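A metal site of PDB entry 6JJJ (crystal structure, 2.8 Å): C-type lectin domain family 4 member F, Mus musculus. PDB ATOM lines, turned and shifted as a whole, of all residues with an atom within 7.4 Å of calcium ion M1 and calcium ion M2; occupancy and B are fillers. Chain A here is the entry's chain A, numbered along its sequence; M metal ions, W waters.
The side-chain carboxylate (OE1) of Glu 126 is bound to calcium ion M1 (2.2 Å). Calcium ion M1 is bound by water W1, at 2.3 Å. The side-chain amide oxygen (OD1) of Asn 136 binds calcium ion M1 (2.4 Å). The side-chain carboxylate (OD1) of Asp 116 binds calcium ion M1. Calcium ion M1 is bound by O of Asp 137, 2.6 Å away. OD1 of Asp 137 binds calcium ion M1, at 2.8 Å. Slightly farther from calcium ion M1 lies OE2 of Glu 126 (3.0 Å). Slightly farther from calcium ion M1 lies OD2 of Asp 116 (3.1 Å).
Residues that only touch calcium ion M1: Gln 114 (3.4 Å). Five residues have an atom within 4 Å of calcium ion M1: Gln 114, Asp 116, Glu 126, Asn 136 and Asp 137. The nearest printed residue that does not touch calcium ion M1 is Trp 118 (4.6 Å).
Along chain A the residues within 4 Å of calcium ion M2 span positions 86 to 127.
Calcium ion M2 is bound by OE2 of Glu 90, 2.1 Å away. Calcium ion M2 is bound by OD1 of Asp 86. OD1 of Asp 127 binds calcium ion M2, at 2.3 Å. Calcium ion M2 is bound by OD2 of Asp 86 (2.3 Å). The backbone carbonyl oxygen (O) of Glu 126 binds calcium ion M2 (2.4 Å). OD1 of Asn 117 binds calcium ion M2 (2.8 Å). Calcium ion M2 has six donor atoms within binding distance. Slightly farther from calcium ion M2 lies the side-chain carboxylate (OE1) of Glu 90 (3.0 Å).
The side-chain carboxylate (OE1) of Glu 126 sits close to the backbone NH (N) of Trp 118. The side-chain carboxylate (OE2) of Glu 126 sits at hydrogen-bond distance from a ring nitrogen (NE2) of His 120 (3.1 Å). The backbone NH (N) of Asp 127 is in hydrogen-bond range of the backbone carbonyl oxygen (O) of Met 138 (3.1 Å). The side-chain amide oxygen (OD1) of Asn 136 sits close to the side-chain amide nitrogen (NE2) of Gln 114 (2.8 Å). The backbone NH (N) of Asn 136 is in hydrogen-bond range of the backbone carbonyl oxygen (O) of His 130 (3.2 Å). The side-chain amide oxygen (OE1) of Gln 114 sits at hydrogen-bond distance from the backbone NH (N) of Asp 116 (2.4 Å). The backbone NH (N) of Asn 117 lies within hydrogen-bond range of the side-chain carboxylate (OD2) of Asp 137 (2.8 Å). OD1 of Asp 137 lies close to OE1 of Gln 114 (3.0 Å).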
ATOM      1  N   THR A  85     -21.358  26.382  21.991  1.00  0.00           N
ATOM      2  CA  THR A  85     -21.423  25.662  20.734  1.00  0.00           C
ATOM      3  C   THR A  85     -20.177  25.928  19.907  1.00  0.00           C
ATOM      4  O   THR A  85     -19.619  27.028  19.938  1.00  0.00           O
ATOM      5  CB  THR A  85     -22.680  26.043  19.934  1.00  0.00           C
ATOM      6  OG1 THR A  85     -22.616  25.439  18.629  1.00  0.00           O
ATOM      7  CG2 THR A  85     -22.783  27.552  19.794  1.00  0.00           C
ATOM      8  N   ASP A  86     -19.769  24.920  19.135  1.00  0.00           N
ATOM      9  CA  ASP A  86     -18.671  25.010  18.179  1.00  0.00           C
ATOM     10  C   ASP A  86     -19.245  24.803  16.770  1.00  0.00           C
ATOM     11  O   ASP A  86     -18.645  24.172  15.907  1.00  0.00           O
ATOM     12  CB  ASP A  86     -17.569  24.001  18.476  1.00  0.00           C
ATOM     13  CG  ASP A  86     -18.013  22.561  18.278  1.00  0.00           C
ATOM     14  OD1 ASP A  86     -19.210  22.330  18.010  1.00  0.00           O
ATOM     15  OD2 ASP A  86     -17.151  21.661  18.396  1.00  0.00           O
ATOM     16  N   GLN A  87     -20.435  25.334  16.553  1.00  0.00           N
ATOM     17  CA  GLN A  87     -21.161  25.203  15.297  1.00  0.00           C
ATOM     18  C   GLN A  87     -20.439  25.873  14.138  1.00  0.00           C
ATOM     19  O   GLN A  87     -19.828  25.169  13.333  1.00  0.00           O
ATOM     20  CB  GLN A  87     -22.545  25.779  15.509  1.00  0.00           C
ATOM     21  CG  GLN A  87     -23.480  25.773  14.334  1.00  0.00           C
ATOM     22  CD  GLN A  87     -24.839  26.319  14.726  1.00  0.00           C
ATOM     23  OE1 GLN A  87     -25.831  25.600  14.687  1.00  0.00           O
ATOM     24  NE2 GLN A  87     -24.870  27.577  15.155  1.00  0.00           N
ATOM     25  N   THR A  89     -17.472  26.914  13.446  1.00  0.00           N
ATOM     26  CA  THR A  89     -16.322  26.072  13.106  1.00  0.00           C
ATOM     27  C   THR A  89     -16.184  24.990  14.167  1.00  0.00           C
ATOM     28  O   THR A  89     -16.285  25.275  15.361  1.00  0.00           O
ATOM     29  CB  THR A  89     -15.028  26.880  13.006  1.00  0.00           C
ATOM     30  OG1 THR A  89     -14.353  26.855  14.265  1.00  0.00           O
ATOM     31  CG2 THR A  89     -15.319  28.316  12.622  1.00  0.00           C
ATOM     32  N   GLU A  90     -15.942  23.753  13.724  1.00  0.00           N
ATOM     33  CA  GLU A  90     -15.965  22.615  14.633  1.00  0.00           C
ATOM     34  C   GLU A  90     -14.969  22.760  15.775  1.00  0.00           C
ATOM     35  O   GLU A  90     -15.162  22.158  16.843  1.00  0.00           O
ATOM     36  CB  GLU A  90     -15.691  21.332  13.862  1.00  0.00           C
ATOM     37  CG  GLU A  90     -15.780  20.081  14.701  1.00  0.00           C
ATOM     38  CD  GLU A  90     -17.101  19.966  15.418  1.00  0.00           C
ATOM     39  OE1 GLU A  90     -18.123  20.424  14.875  1.00  0.00           O
ATOM     40  OE2 GLU A  90     -17.106  19.419  16.541  1.00  0.00           O
ATOM     41  N   GLY A  91     -13.905  23.521  15.578  1.00  0.00           N
ATOM     42  CA  GLY A  91     -12.884  23.636  16.599  1.00  0.00           C
ATOM     43  C   GLY A  91     -13.235  24.607  17.706  1.00  0.00           C
ATOM     44  O   GLY A  91     -13.257  24.227  18.881  1.00  0.00           O
ATOM     45  N   ILE A  92     -13.524  25.841  17.335  1.00  0.00           N
ATOM     46  CA  ILE A  92     -13.696  26.908  18.332  1.00  0.00           C
ATOM     47  C   ILE A  92     -15.097  26.813  18.915  1.00  0.00           C
ATOM     48  O   ILE A  92     -16.084  26.713  18.185  1.00  0.00           O
ATOM     49  CB  ILE A  92     -13.444  28.283  17.693  1.00  0.00           C
ATOM     50  CG1 ILE A  92     -14.637  28.686  16.808  1.00  0.00           C
ATOM     51  CG2 ILE A  92     -12.152  28.270  16.894  1.00  0.00           C
ATOM     52  CD1 ILE A  92     -14.397  29.913  15.955  1.00  0.00           C
ATOM     53  N   TRP A  93     -15.173  26.861  20.239  1.00  0.00           N
ATOM     54  CA  TRP A  93     -16.426  27.064  20.952  1.00  0.00           C
ATOM     55  C   TRP A  93     -16.583  28.550  21.242  1.00  0.00           C
ATOM     56  O   TRP A  93     -15.629  29.321  21.214  1.00  0.00           O
ATOM     57  CB  TRP A  93     -16.453  26.282  22.266  1.00  0.00           C
ATOM     58  CG  TRP A  93     -16.277  24.800  22.095  1.00  0.00           C
ATOM     59  CD1 TRP A  93     -15.097  24.121  22.089  1.00  0.00           C
ATOM     60  CD2 TRP A  93     -17.315  23.821  21.957  1.00  0.00           C
ATOM     61  NE1 TRP A  93     -15.331  22.769  21.934  1.00  0.00           N
ATOM     62  CE2 TRP A  93     -16.686  22.560  21.854  1.00  0.00           C
ATOM     63  CE3 TRP A  93     -18.709  23.879  21.901  1.00  0.00           C
ATOM     64  CZ2 TRP A  93     -17.400  21.383  21.691  1.00  0.00           C
ATOM     65  CZ3 TRP A  93     -19.415  22.702  21.750  1.00  0.00           C
ATOM     66  CH2 TRP A  93     -18.758  21.474  21.648  1.00  0.00           C
ATOM     67  N   ASN A 113     -13.952  12.602  29.733  1.00  0.00           N
ATOM     68  CA  ASN A 113     -13.455  12.649  28.364  1.00  0.00           C
ATOM     69  C   ASN A 113     -14.541  13.341  27.533  1.00  0.00           C
ATOM     70  O   ASN A 113     -15.445  12.683  27.003  1.00  0.00           O
ATOM     71  CB  ASN A 113     -13.101  11.259  27.823  1.00  0.00           C
ATOM     72  CG  ASN A 113     -14.211  10.243  27.995  1.00  0.00           C
ATOM     73  OD1 ASN A 113     -15.119  10.157  27.162  1.00  0.00           O
ATOM     74  ND2 ASN A 113     -14.141   9.465  29.065  1.00  0.00           N
ATOM     75  N   GLN A 114     -14.466  14.674  27.436  1.00  0.00           N
ATOM     76  CA  GLN A 114     -15.495  15.471  26.786  1.00  0.00           C
ATOM     77  C   GLN A 114     -14.899  16.837  26.488  1.00  0.00           C
ATOM     78  O   GLN A 114     -14.100  17.327  27.297  1.00  0.00           O
ATOM     79  CB  GLN A 114     -16.731  15.614  27.684  1.00  0.00           C
ATOM     80  CG  GLN A 114     -18.064  15.751  26.966  1.00  0.00           C
ATOM     81  CD  GLN A 114     -18.346  14.606  26.018  1.00  0.00           C
ATOM     82  OE1 GLN A 114     -17.964  14.649  24.845  1.00  0.00           O
ATOM     83  NE2 GLN A 114     -19.022  13.572  26.512  1.00  0.00           N
ATOM     84  N   PRO A 115     -15.245  17.480  25.363  1.00  0.00           N
ATOM     85  CA  PRO A 115     -16.192  17.042  24.321  1.00  0.00           C
ATOM     86  C   PRO A 115     -15.661  15.913  23.436  1.00  0.00           C
ATOM     87  O   PRO A 115     -14.451  15.803  23.230  1.00  0.00           O
ATOM     88  CB  PRO A 115     -16.408  18.313  23.486  1.00  0.00           C
ATOM     89  CG  PRO A 115     -15.135  19.092  23.658  1.00  0.00           C
ATOM     90  CD  PRO A 115     -14.664  18.806  25.057  1.00  0.00           C
ATOM     91  N   ASP A 116     -16.576  15.091  22.919  1.00  0.00           N
ATOM     92  CA  ASP A 116     -16.223  13.995  22.030  1.00  0.00           C
ATOM     93  C   ASP A 116     -16.691  14.213  20.605  1.00  0.00           C
ATOM     94  O   ASP A 116     -16.129  13.603  19.682  1.00  0.00           O
ATOM     95  CB  ASP A 116     -16.800  12.677  22.546  1.00  0.00           C
ATOM     96  CG  ASP A 116     -18.301  12.729  22.731  1.00  0.00           C
ATOM     97  OD1 ASP A 116     -18.881  13.814  22.519  1.00  0.00           O
ATOM     98  OD2 ASP A 116     -18.902  11.700  23.100  1.00  0.00           O
ATOM     99  N   ASN A 117     -17.700  15.064  20.392  1.00  0.00           N
ATOM    100  CA  ASN A 117     -18.226  15.331  19.049  1.00  0.00           C
ATOM    101  C   ASN A 117     -18.738  14.043  18.411  1.00  0.00           C
ATOM    102  O   ASN A 117     -18.474  13.763  17.230  1.00  0.00           O
ATOM    103  CB  ASN A 117     -17.174  16.005  18.166  1.00  0.00           C
ATOM    104  CG  ASN A 117     -17.794  16.763  17.020  1.00  0.00           C
ATOM    105  OD1 ASN A 117     -18.858  17.354  17.163  1.00  0.00           O
ATOM    106  ND2 ASN A 117     -17.114  16.763  15.871  1.00  0.00           N
ATOM    107  N   TRP A 118     -19.459  13.258  19.186  1.00  0.00           N
ATOM    108  CA  TRP A 118     -19.907  11.944  18.739  1.00  0.00           C
ATOM    109  C   TRP A 118     -20.771  12.071  17.490  1.00  0.00           C
ATOM    110  O   TRP A 118     -21.486  13.060  17.306  1.00  0.00           O
ATOM    111  CB  TRP A 118     -20.690  11.251  19.859  1.00  0.00           C
ATOM    112  CG  TRP A 118     -20.853   9.787  19.671  1.00  0.00           C
ATOM    113  CD1 TRP A 118     -19.875   8.832  19.721  1.00  0.00           C
ATOM    114  CD2 TRP A 118     -22.071   9.079  19.427  1.00  0.00           C
ATOM    115  NE1 TRP A 118     -20.405   7.585  19.518  1.00  0.00           N
ATOM    116  CE2 TRP A 118     -21.758   7.706  19.334  1.00  0.00           C
ATOM    117  CE3 TRP A 118     -23.406   9.481  19.283  1.00  0.00           C
ATOM    118  CZ2 TRP A 118     -22.727   6.741  19.091  1.00  0.00           C
ATOM    119  CZ3 TRP A 118     -24.364   8.506  19.042  1.00  0.00           C
ATOM    120  CH2 TRP A 118     -24.021   7.156  18.948  1.00  0.00           C
ATOM    121  N   HIS A 120     -23.899  11.051  15.584  1.00  0.00           N
ATOM    122  CA  HIS A 120     -25.195  10.453  15.858  1.00  0.00           C
ATOM    123  C   HIS A 120     -25.734   9.735  14.620  1.00  0.00           C
ATOM    124  O   HIS A 120     -25.274   9.944  13.494  1.00  0.00           O
ATOM    125  CB  HIS A 120     -26.188  11.514  16.323  1.00  0.00           C
ATOM    126  CG  HIS A 120     -26.064  11.875  17.771  1.00  0.00           C
ATOM    127  ND1 HIS A 120     -27.015  11.550  18.714  1.00  0.00           N
ATOM    128  CD2 HIS A 120     -25.074  12.513  18.447  1.00  0.00           C
ATOM    129  CE1 HIS A 120     -26.635  11.984  19.894  1.00  0.00           C
ATOM    130  NE2 HIS A 120     -25.451  12.572  19.765  1.00  0.00           N
ATOM    131  N   ARG A 125     -23.358  15.567  13.999  1.00  0.00           N
ATOM    132  CA  ARG A 125     -22.274  15.590  14.966  1.00  0.00           C
ATOM    133  C   ARG A 125     -22.822  16.240  16.240  1.00  0.00           C
ATOM    134  O   ARG A 125     -24.033  16.402  16.399  1.00  0.00           O
ATOM    135  CB  ARG A 125     -21.076  16.349  14.400  1.00  0.00           C
ATOM    136  CG  ARG A 125     -20.503  15.732  13.136  1.00  0.00           C
ATOM    137  CD  ARG A 125     -19.991  14.318  13.352  1.00  0.00           C
ATOM    138  NE  ARG A 125     -19.149  13.899  12.230  1.00  0.00           N
ATOM    139  CZ  ARG A 125     -19.618  13.393  11.092  1.00  0.00           C
ATOM    140  NH1 ARG A 125     -20.919  13.257  10.908  1.00  0.00           N
ATOM    141  NH2 ARG A 125     -18.775  13.024  10.141  1.00  0.00           N
ATOM    142  N   GLU A 126     -21.942  16.628  17.166  1.00  0.00           N
ATOM    143  CA  GLU A 126     -22.357  17.293  18.404  1.00  0.00           C
ATOM    144  C   GLU A 126     -21.764  18.687  18.450  1.00  0.00           C
ATOM    145  O   GLU A 126     -20.543  18.842  18.541  1.00  0.00           O
ATOM    146  CB  GLU A 126     -21.937  16.470  19.615  1.00  0.00           C
ATOM    147  CG  GLU A 126     -22.595  15.092  19.688  1.00  0.00           C
ATOM    148  CD  GLU A 126     -22.280  14.375  20.985  1.00  0.00           C
ATOM    149  OE1 GLU A 126     -21.153  14.543  21.489  1.00  0.00           O
ATOM    150  OE2 GLU A 126     -23.163  13.651  21.494  1.00  0.00           O
ATOM    151  N   ASP A 127     -22.635  19.704  18.372  1.00  0.00           N
ATOM    152  CA  ASP A 127     -22.198  21.106  18.377  1.00  0.00           C
ATOM    153  C   ASP A 127     -22.963  21.942  19.402  1.00  0.00           C
ATOM    154  O   ASP A 127     -22.980  23.175  19.292  1.00  0.00           O
ATOM    155  CB  ASP A 127     -22.346  21.725  16.991  1.00  0.00           C
ATOM    156  CG  ASP A 127     -21.524  21.017  15.952  1.00  0.00           C
ATOM    157  OD1 ASP A 127     -20.444  20.497  16.297  1.00  0.00           O
ATOM    158  OD2 ASP A 127     -21.948  20.991  14.776  1.00  0.00           O
ATOM    159  N   CYS A 128     -23.617  21.311  20.375  1.00  0.00           N
ATOM    160  CA  CYS A 128     -24.370  22.027  21.392  1.00  0.00           C
ATOM    161  C   CYS A 128     -24.121  21.351  22.728  1.00  0.00           C
ATOM    162  O   CYS A 128     -23.908  20.139  22.799  1.00  0.00           O
ATOM    163  CB  CYS A 128     -25.862  22.063  21.059  1.00  0.00           C
ATOM    164  SG  CYS A 128     -26.273  23.122  19.632  1.00  0.00           S
ATOM    165  N   HIS A 130     -25.132  20.723  26.858  1.00  0.00           N
ATOM    166  CA  HIS A 130     -26.088  20.719  27.953  1.00  0.00           C
ATOM    167  C   HIS A 130     -25.348  20.326  29.237  1.00  0.00           C
ATOM    168  O   HIS A 130     -24.168  19.970  29.209  1.00  0.00           O
ATOM    169  CB  HIS A 130     -27.268  19.775  27.676  1.00  0.00           C
ATOM    170  CG  HIS A 130     -26.888  18.348  27.430  1.00  0.00           C
ATOM    171  ND1 HIS A 130     -27.684  17.480  26.722  1.00  0.00           N
ATOM    172  CD2 HIS A 130     -25.801  17.635  27.811  1.00  0.00           C
ATOM    173  CE1 HIS A 130     -27.106  16.302  26.666  1.00  0.00           C
ATOM    174  NE2 HIS A 130     -25.960  16.362  27.321  1.00  0.00           N
ATOM    175  N   TRP A 135     -20.433  19.440  31.708  1.00  0.00           N
ATOM    176  CA  TRP A 135     -20.861  19.708  30.350  1.00  0.00           C
ATOM    177  C   TRP A 135     -20.729  18.468  29.473  1.00  0.00           C
ATOM    178  O   TRP A 135     -19.941  17.561  29.746  1.00  0.00           O
ATOM    179  CB  TRP A 135     -20.045  20.834  29.736  1.00  0.00           C
ATOM    180  CG  TRP A 135     -20.132  22.117  30.473  1.00  0.00           C
ATOM    181  CD1 TRP A 135     -20.971  22.401  31.511  1.00  0.00           C
ATOM    182  CD2 TRP A 135     -19.370  23.295  30.233  1.00  0.00           C
ATOM    183  NE1 TRP A 135     -20.764  23.693  31.934  1.00  0.00           N
ATOM    184  CE2 TRP A 135     -19.797  24.260  31.163  1.00  0.00           C
ATOM    185  CE3 TRP A 135     -18.374  23.623  29.314  1.00  0.00           C
ATOM    186  CZ2 TRP A 135     -19.246  25.540  31.208  1.00  0.00           C
ATOM    187  CZ3 TRP A 135     -17.833  24.902  29.357  1.00  0.00           C
ATOM    188  CH2 TRP A 135     -18.270  25.846  30.292  1.00  0.00           C
ATOM    189  N   ASN A 136     -21.536  18.428  28.411  1.00  0.00           N
ATOM    190  CA  ASN A 136     -21.400  17.410  27.378  1.00  0.00           C
ATOM    191  C   ASN A 136     -21.888  18.011  26.066  1.00  0.00           C
ATOM    192  O   ASN A 136     -23.008  18.539  26.012  1.00  0.00           O
ATOM    193  CB  ASN A 136     -22.199  16.143  27.704  1.00  0.00           C
ATOM    194  CG  ASN A 136     -22.279  15.184  26.535  1.00  0.00           C
ATOM    195  OD1 ASN A 136     -21.303  14.995  25.802  1.00  0.00           O
ATOM    196  ND2 ASN A 136     -23.444  14.579  26.335  1.00  0.00           N
ATOM    197  N   ASP A 137     -21.066  17.948  25.023  1.00  0.00           N
ATOM    198  CA  ASP A 137     -21.509  18.382  23.707  1.00  0.00           C
ATOM    199  C   ASP A 137     -22.505  17.363  23.161  1.00  0.00           C
ATOM    200  O   ASP A 137     -22.379  16.162  23.397  1.00  0.00           O
ATOM    201  CB  ASP A 137     -20.331  18.599  22.764  1.00  0.00           C
ATOM    202  CG  ASP A 137     -19.632  17.313  22.376  1.00  0.00           C
ATOM    203  OD1 ASP A 137     -19.726  16.310  23.123  1.00  0.00           O
ATOM    204  OD2 ASP A 137     -18.987  17.315  21.313  1.00  0.00           O
ATOM    205  N   MET A 138     -23.509  17.845  22.437  1.00  0.00           N
ATOM    206  CA  MET A 138     -24.658  17.030  22.087  1.00  0.00           C
ATOM    207  C   MET A 138     -25.179  17.450  20.718  1.00  0.00           C
ATOM    208  O   MET A 138     -24.897  18.556  20.239  1.00  0.00           O
ATOM    209  CB  MET A 138     -25.755  17.175  23.158  1.00  0.00           C
ATOM    210  CG  MET A 138     -27.012  16.374  22.894  1.00  0.00           C
ATOM    211  SD  MET A 138     -26.651  14.602  22.819  1.00  0.00           S
ATOM    212  CE  MET A 138     -28.208  13.966  22.199  1.00  0.00           C
ATOM    213  N   ALA A 139     -25.936  16.550  20.101  1.00  0.00           N
ATOM    214  CA  ALA A 139     -26.591  16.870  18.833  1.00  0.00           C
ATOM    215  C   ALA A 139     -27.625  17.962  19.061  1.00  0.00           C
ATOM    216  O   ALA A 139     -28.497  17.851  19.919  1.00  0.00           O
ATOM    217  CB  ALA A 139     -27.259  15.623  18.260  1.00  0.00           C
HETATM  218 CA    CA M   1     -21.075  13.909  23.624  1.00  0.00          CA
HETATM  219 CA    CA M   2     -18.723  20.128  17.753  1.00  0.00          CA
HETATM  220  O   HOH W   1     -21.529  11.820  24.414  1.00  0.00           O
